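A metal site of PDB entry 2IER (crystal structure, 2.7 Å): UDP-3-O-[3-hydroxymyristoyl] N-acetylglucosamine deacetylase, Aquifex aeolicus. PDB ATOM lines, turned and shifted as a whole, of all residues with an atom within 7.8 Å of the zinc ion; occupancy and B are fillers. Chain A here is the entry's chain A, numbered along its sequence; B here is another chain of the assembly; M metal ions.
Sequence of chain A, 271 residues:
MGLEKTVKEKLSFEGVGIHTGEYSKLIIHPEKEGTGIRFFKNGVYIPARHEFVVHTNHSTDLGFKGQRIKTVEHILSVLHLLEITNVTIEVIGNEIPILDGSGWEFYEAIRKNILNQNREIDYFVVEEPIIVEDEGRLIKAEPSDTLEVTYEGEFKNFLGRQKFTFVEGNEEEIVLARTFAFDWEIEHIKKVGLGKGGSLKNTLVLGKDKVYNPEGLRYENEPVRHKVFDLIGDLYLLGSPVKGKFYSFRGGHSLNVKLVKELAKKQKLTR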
ATOM      1  N   GLY A   2     -31.520   5.493   4.954  1.00  0.00           N
ATOM      2  CA  GLY A   2     -31.111   4.066   4.916  1.00  0.00           C
ATOM      3  C   GLY A   2     -29.835   3.872   4.122  1.00  0.00           C
ATOM      4  O   GLY A   2     -29.445   4.733   3.337  1.00  0.00           O
ATOM      5  N   LEU A   3     -29.193   2.739   4.331  1.00  0.00           N
ATOM      6  CA  LEU A   3     -27.948   2.426   3.624  1.00  0.00           C
ATOM      7  C   LEU A   3     -28.237   1.720   2.306  1.00  0.00           C
ATOM      8  O   LEU A   3     -29.226   1.011   2.190  1.00  0.00           O
ATOM      9  CB  LEU A   3     -27.061   1.534   4.499  1.00  0.00           C
ATOM     10  CG  LEU A   3     -26.706   2.106   5.873  1.00  0.00           C
ATOM     11  CD1 LEU A   3     -25.944   1.065   6.694  1.00  0.00           C
ATOM     12  CD2 LEU A   3     -25.883   3.377   5.689  1.00  0.00           C
ATOM     13  N   GLU A   4     -27.378   1.918   1.318  1.00  0.00           N
ATOM     14  CA  GLU A   4     -27.570   1.243   0.037  1.00  0.00           C
ATOM     15  C   GLU A   4     -27.523  -0.246   0.301  1.00  0.00           C
ATOM     16  O   GLU A   4     -26.864  -0.715   1.221  1.00  0.00           O
ATOM     17  CB  GLU A   4     -26.462   1.615  -0.945  1.00  0.00           C
ATOM     18  CG  GLU A   4     -26.330   3.085  -1.217  1.00  0.00           C
ATOM     19  CD  GLU A   4     -25.666   3.374  -2.546  1.00  0.00           C
ATOM     20  OE1 GLU A   4     -24.746   2.619  -2.957  1.00  0.00           O
ATOM     21  OE2 GLU A   4     -26.069   4.365  -3.195  1.00  0.00           O
ATOM     22  N   LYS A   5     -28.240  -1.021  -0.501  1.00  0.00           N
ATOM     23  CA  LYS A   5     -28.246  -2.461  -0.314  1.00  0.00           C
ATOM     24  C   LYS A   5     -28.088  -3.174  -1.648  1.00  0.00           C
ATOM     25  O   LYS A   5     -28.369  -2.615  -2.713  1.00  0.00           O
ATOM     26  CB  LYS A   5     -29.545  -2.898   0.356  1.00  0.00           C
ATOM     27  CG  LYS A   5     -29.851  -2.181   1.652  1.00  0.00           C
ATOM     28  CD  LYS A   5     -31.265  -2.494   2.130  1.00  0.00           C
ATOM     29  CE  LYS A   5     -31.620  -1.686   3.360  1.00  0.00           C
ATOM     30  NZ  LYS A   5     -31.566  -0.225   3.098  1.00  0.00           N
ATOM     31  N   GLU A  83     -35.602  -1.505  -0.989  1.00  0.00           N
ATOM     32  CA  GLU A  83     -34.531  -0.527  -1.060  1.00  0.00           C
ATOM     33  C   GLU A  83     -33.206  -1.138  -1.551  1.00  0.00           C
ATOM     34  O   GLU A  83     -32.125  -0.750  -1.090  1.00  0.00           O
ATOM     35  CB  GLU A  83     -34.344   0.130   0.311  1.00  0.00           C
ATOM     36  CG  GLU A  83     -34.511   1.627   0.296  1.00  0.00           C
ATOM     37  CD  GLU A  83     -34.619   2.240   1.678  1.00  0.00           C
ATOM     38  OE1 GLU A  83     -33.750   1.938   2.535  1.00  0.00           O
ATOM     39  OE2 GLU A  83     -35.565   3.028   1.909  1.00  0.00           O
ATOM     40  N   ARG A 119     -22.858   3.082   2.247  1.00  0.00           N
ATOM     41  CA  ARG A 119     -23.205   4.354   1.665  1.00  0.00           C
ATOM     42  C   ARG A 119     -24.652   4.657   1.973  1.00  0.00           C
ATOM     43  O   ARG A 119     -25.513   3.775   1.917  1.00  0.00           O
ATOM     44  CB  ARG A 119     -22.973   4.349   0.154  1.00  0.00           C
ATOM     45  CG  ARG A 119     -23.148   5.707  -0.495  1.00  0.00           C
ATOM     46  CD  ARG A 119     -22.744   5.722  -1.969  1.00  0.00           C
ATOM     47  NE  ARG A 119     -21.337   5.407  -2.147  1.00  0.00           N
ATOM     48  CZ  ARG A 119     -20.678   5.551  -3.304  1.00  0.00           C
ATOM     49  NH1 ARG A 119     -21.299   6.009  -4.376  1.00  0.00           N
ATOM     50  NH2 ARG A 119     -19.400   5.221  -3.370  1.00  0.00           N
ATOM     51  N   GLU A 120     -24.908   5.893   2.335  1.00  0.00           N
ATOM     52  CA  GLU A 120     -26.255   6.346   2.636  1.00  0.00           C
ATOM     53  C   GLU A 120     -26.952   6.500   1.290  1.00  0.00           C
ATOM     54  O   GLU A 120     -26.354   6.985   0.318  1.00  0.00           O
ATOM     55  CB  GLU A 120     -26.208   7.681   3.370  1.00  0.00           C
ATOM     56  CG  GLU A 120     -27.540   8.393   3.529  1.00  0.00           C
ATOM     57  CD  GLU A 120     -28.495   7.660   4.437  1.00  0.00           C
ATOM     58  OE1 GLU A 120     -28.014   6.931   5.326  1.00  0.00           O
ATOM     59  OE2 GLU A 120     -29.721   7.824   4.290  1.00  0.00           O
ATOM     60  N   ILE A 121     -28.208   6.082   1.243  1.00  0.00           N
ATOM     61  CA  ILE A 121     -28.997   6.193   0.029  1.00  0.00           C
ATOM     62  C   ILE A 121     -29.237   7.661  -0.251  1.00  0.00           C
ATOM     63  O   ILE A 121     -29.484   8.435   0.664  1.00  0.00           O
ATOM     64  CB  ILE A 121     -30.374   5.494   0.195  1.00  0.00           C
ATOM     65  CG1 ILE A 121     -30.184   3.966   0.206  1.00  0.00           C
ATOM     66  CG2 ILE A 121     -31.329   5.910  -0.916  1.00  0.00           C
ATOM     67  CD1 ILE A 121     -31.466   3.201   0.474  1.00  0.00           C
ATOM     68  N   TYR A 123     -31.803   9.428  -1.738  1.00  0.00           N
ATOM     69  CA  TYR A 123     -33.182   9.346  -2.221  1.00  0.00           C
ATOM     70  C   TYR A 123     -33.614  10.441  -3.170  1.00  0.00           C
ATOM     71  O   TYR A 123     -33.097  11.553  -3.144  1.00  0.00           O
ATOM     72  CB  TYR A 123     -34.172   9.357  -1.039  1.00  0.00           C
ATOM     73  CG  TYR A 123     -33.978   8.229  -0.058  1.00  0.00           C
ATOM     74  CD1 TYR A 123     -33.007   8.298   0.925  1.00  0.00           C
ATOM     75  CD2 TYR A 123     -34.790   7.091  -0.117  1.00  0.00           C
ATOM     76  CE1 TYR A 123     -32.841   7.270   1.860  1.00  0.00           C
ATOM     77  CE2 TYR A 123     -34.636   6.050   0.802  1.00  0.00           C
ATOM     78  CZ  TYR A 123     -33.664   6.147   1.791  1.00  0.00           C
ATOM     79  OH  TYR A 123     -33.533   5.136   2.715  1.00  0.00           O
ATOM     80  N   LYS B  10     -32.374  14.106   8.653  1.00  0.00           N
ATOM     81  CA  LYS B  10     -31.156  13.312   8.701  1.00  0.00           C
ATOM     82  C   LYS B  10     -29.944  14.208   8.812  1.00  0.00           C
ATOM     83  O   LYS B  10     -29.862  15.238   8.137  1.00  0.00           O
ATOM     84  CB  LYS B  10     -30.986  12.480   7.433  1.00  0.00           C
ATOM     85  CG  LYS B  10     -32.115  11.532   7.117  1.00  0.00           C
ATOM     86  CD  LYS B  10     -31.753  10.644   5.919  1.00  0.00           C
ATOM     87  CE  LYS B  10     -31.273  11.460   4.720  1.00  0.00           C
ATOM     88  NZ  LYS B  10     -30.787  10.594   3.601  1.00  0.00           N
ATOM     89  N   LEU B  26     -21.809   8.267   9.781  1.00  0.00           N
ATOM     90  CA  LEU B  26     -23.021   8.152  10.590  1.00  0.00           C
ATOM     91  C   LEU B  26     -24.137   8.890   9.884  1.00  0.00           C
ATOM     92  O   LEU B  26     -23.893   9.883   9.197  1.00  0.00           O
ATOM     93  CB  LEU B  26     -22.878   8.837  11.930  1.00  0.00           C
ATOM     94  CG  LEU B  26     -21.766   8.493  12.900  1.00  0.00           C
ATOM     95  CD1 LEU B  26     -21.914   9.402  14.116  1.00  0.00           C
ATOM     96  CD2 LEU B  26     -21.857   7.027  13.289  1.00  0.00           C
ATOM     97  N   ILE B  27     -25.351   8.415  10.067  1.00  0.00           N
ATOM     98  CA  ILE B  27     -26.508   9.089   9.518  1.00  0.00           C
ATOM     99  C   ILE B  27     -27.522   9.011  10.644  1.00  0.00           C
ATOM    100  O   ILE B  27     -28.028   7.934  10.965  1.00  0.00           O
ATOM    101  CB  ILE B  27     -27.087   8.388   8.264  1.00  0.00           C
ATOM    102  CG1 ILE B  27     -26.040   8.306   7.150  1.00  0.00           C
ATOM    103  CG2 ILE B  27     -28.311   9.164   7.779  1.00  0.00           C
ATOM    104  CD1 ILE B  27     -25.012   7.193   7.322  1.00  0.00           C
ATOM    105  N   ILE B  28     -27.782  10.149  11.277  1.00  0.00           N
ATOM    106  CA  ILE B  28     -28.735  10.173  12.374  1.00  0.00           C
ATOM    107  C   ILE B  28     -30.138  10.345  11.818  1.00  0.00           C
ATOM    108  O   ILE B  28     -30.458  11.359  11.198  1.00  0.00           O
ATOM    109  CB  ILE B  28     -28.387  11.292  13.344  1.00  0.00           C
ATOM    110  CG1 ILE B  28     -26.938  11.123  13.810  1.00  0.00           C
ATOM    111  CG2 ILE B  28     -29.325  11.249  14.537  1.00  0.00           C
ATOM    112  CD1 ILE B  28     -26.439  12.234  14.705  1.00  0.00           C
ATOM    113  N   HIS B  29     -30.966   9.332  12.044  1.00  0.00           N
ATOM    114  CA  HIS B  29     -32.339   9.316  11.571  1.00  0.00           C
ATOM    115  C   HIS B  29     -33.368   9.631  12.628  1.00  0.00           C
ATOM    116  O   HIS B  29     -33.268   9.196  13.780  1.00  0.00           O
ATOM    117  CB  HIS B  29     -32.667   7.939  10.974  1.00  0.00           C
ATOM    118  CG  HIS B  29     -31.984   7.669   9.669  1.00  0.00           C
ATOM    119  ND1 HIS B  29     -32.324   8.326   8.511  1.00  0.00           N
ATOM    120  CD2 HIS B  29     -30.977   6.822   9.350  1.00  0.00           C
ATOM    121  CE1 HIS B  29     -31.549   7.904   7.526  1.00  0.00           C
ATOM    122  NE2 HIS B  29     -30.722   6.994   8.018  1.00  0.00           N
ATOM    123  N   PHE B  40     -27.610   1.403  14.302  1.00  0.00           N
ATOM    124  CA  PHE B  40     -27.951   0.443  13.269  1.00  0.00           C
ATOM    125  C   PHE B  40     -26.699   0.138  12.454  1.00  0.00           C
ATOM    126  O   PHE B  40     -26.083   1.042  11.882  1.00  0.00           O
ATOM    127  CB  PHE B  40     -29.024   0.989  12.339  1.00  0.00           C
ATOM    128  CG  PHE B  40     -29.413   0.036  11.252  1.00  0.00           C
ATOM    129  CD1 PHE B  40     -30.269  -1.026  11.525  1.00  0.00           C
ATOM    130  CD2 PHE B  40     -28.898   0.176   9.970  1.00  0.00           C
ATOM    131  CE1 PHE B  40     -30.609  -1.949  10.540  1.00  0.00           C
ATOM    132  CE2 PHE B  40     -29.227  -0.737   8.969  1.00  0.00           C
ATOM    133  CZ  PHE B  40     -30.081  -1.806   9.257  1.00  0.00           C
ATOM    134  N   THR B  88     -32.120   6.963  15.347  1.00  0.00           N
ATOM    135  CA  THR B  88     -31.449   5.729  14.973  1.00  0.00           C
ATOM    136  C   THR B  88     -30.158   6.203  14.340  1.00  0.00           C
ATOM    137  O   THR B  88     -30.179   6.972  13.365  1.00  0.00           O
ATOM    138  CB  THR B  88     -32.248   4.907  13.939  1.00  0.00           C
ATOM    139  OG1 THR B  88     -33.424   4.379  14.567  1.00  0.00           O
ATOM    140  CG2 THR B  88     -31.406   3.744  13.415  1.00  0.00           C
ATOM    141  N   ILE B  89     -29.034   5.781  14.907  1.00  0.00           N
ATOM    142  CA  ILE B  89     -27.735   6.195  14.399  1.00  0.00           C
ATOM    143  C   ILE B  89     -27.154   5.139  13.472  1.00  0.00           C
ATOM    144  O   ILE B  89     -26.466   4.218  13.912  1.00  0.00           O
ATOM    145  CB  ILE B  89     -26.751   6.456  15.551  1.00  0.00           C
ATOM    146  CG1 ILE B  89     -27.359   7.484  16.513  1.00  0.00           C
ATOM    147  CG2 ILE B  89     -25.422   6.943  14.994  1.00  0.00           C
ATOM    148  CD1 ILE B  89     -26.618   7.584  17.826  1.00  0.00           C
ATOM    149  N   GLU B  90     -27.441   5.272  12.196  1.00  0.00           N
ATOM    150  CA  GLU B  90     -26.923   4.359  11.185  1.00  0.00           C
ATOM    151  C   GLU B  90     -25.407   4.510  11.149  1.00  0.00           C
ATOM    152  O   GLU B  90     -24.898   5.618  11.028  1.00  0.00           O
ATOM    153  CB  GLU B  90     -27.500   4.700   9.827  1.00  0.00           C
ATOM    154  CG  GLU B  90     -28.666   3.848   9.420  1.00  0.00           C
ATOM    155  CD  GLU B  90     -29.270   4.333   8.106  1.00  0.00           C
ATOM    156  OE1 GLU B  90     -28.512   4.688   7.195  1.00  0.00           O
ATOM    157  OE2 GLU B  90     -30.504   4.335   7.990  1.00  0.00           O
ATOM    158  N   VAL B  91     -24.708   3.380  11.235  1.00  0.00           N
ATOM    159  CA  VAL B  91     -23.251   3.419  11.210  1.00  0.00           C
ATOM    160  C   VAL B  91     -22.636   2.638  10.044  1.00  0.00           C
ATOM    161  O   VAL B  91     -22.874   1.440   9.905  1.00  0.00           O
ATOM    162  CB  VAL B  91     -22.636   2.894  12.535  1.00  0.00           C
ATOM    163  CG1 VAL B  91     -21.108   3.057  12.516  1.00  0.00           C
ATOM    164  CG2 VAL B  91     -23.236   3.648  13.719  1.00  0.00           C
ATOM    165  N   ILE B  92     -21.883   3.348   9.212  1.00  0.00           N
ATOM    166  CA  ILE B  92     -21.186   2.743   8.092  1.00  0.00           C
ATOM    167  C   ILE B  92     -19.728   2.622   8.533  1.00  0.00           C
ATOM    168  O   ILE B  92     -18.924   3.533   8.362  1.00  0.00           O
ATOM    169  CB  ILE B  92     -21.246   3.660   6.838  1.00  0.00           C
ATOM    170  CG1 ILE B  92     -22.679   3.754   6.322  1.00  0.00           C
ATOM    171  CG2 ILE B  92     -20.294   3.125   5.758  1.00  0.00           C
ATOM    172  CD1 ILE B  92     -22.849   4.764   5.213  1.00  0.00           C
HETATM  173 ZN    ZN M   1     -29.814   6.322   6.312  1.00  0.00          ZN
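Ile 27 of chain B touches the zinc ion (CG2 to ZN, 3.5 Å).
Five residues have an atom within 4 Å of the zinc ion: Gly 2, Glu 120, Ile 27 of chain B, His 29 of chain B and Glu 90 of chain B.
The nearest printed residue that does not touch the zinc ion is Leu 3 (4.1 Å).
OH of Tyr 123 lies close to N of Gly 2 (3.0 Å).
N of Ile 121 sits at hydrogen-bond distance from O of Gly 2 (2.8 Å).
N of Glu 90 of chain B sits at hydrogen-bond distance from O of Ile 27 of chain B, 3.0 Å away.
The side-chain amino group (NZ) of Lys 10 of chain B lies close to the side-chain carboxylate (OE2) of Glu 120 (3.0 Å).
The zinc ion is bound by NE2 of His 29 of chain B, OE1 of Glu 120, OE1 of Glu 90 of chain B, N of Gly 2 and OE2 of Glu 120.
The zinc ion has five donor atoms within binding distance.
Slightly farther from the zinc ion lies OE2 of Glu 90 of chain B (2.7 Å).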
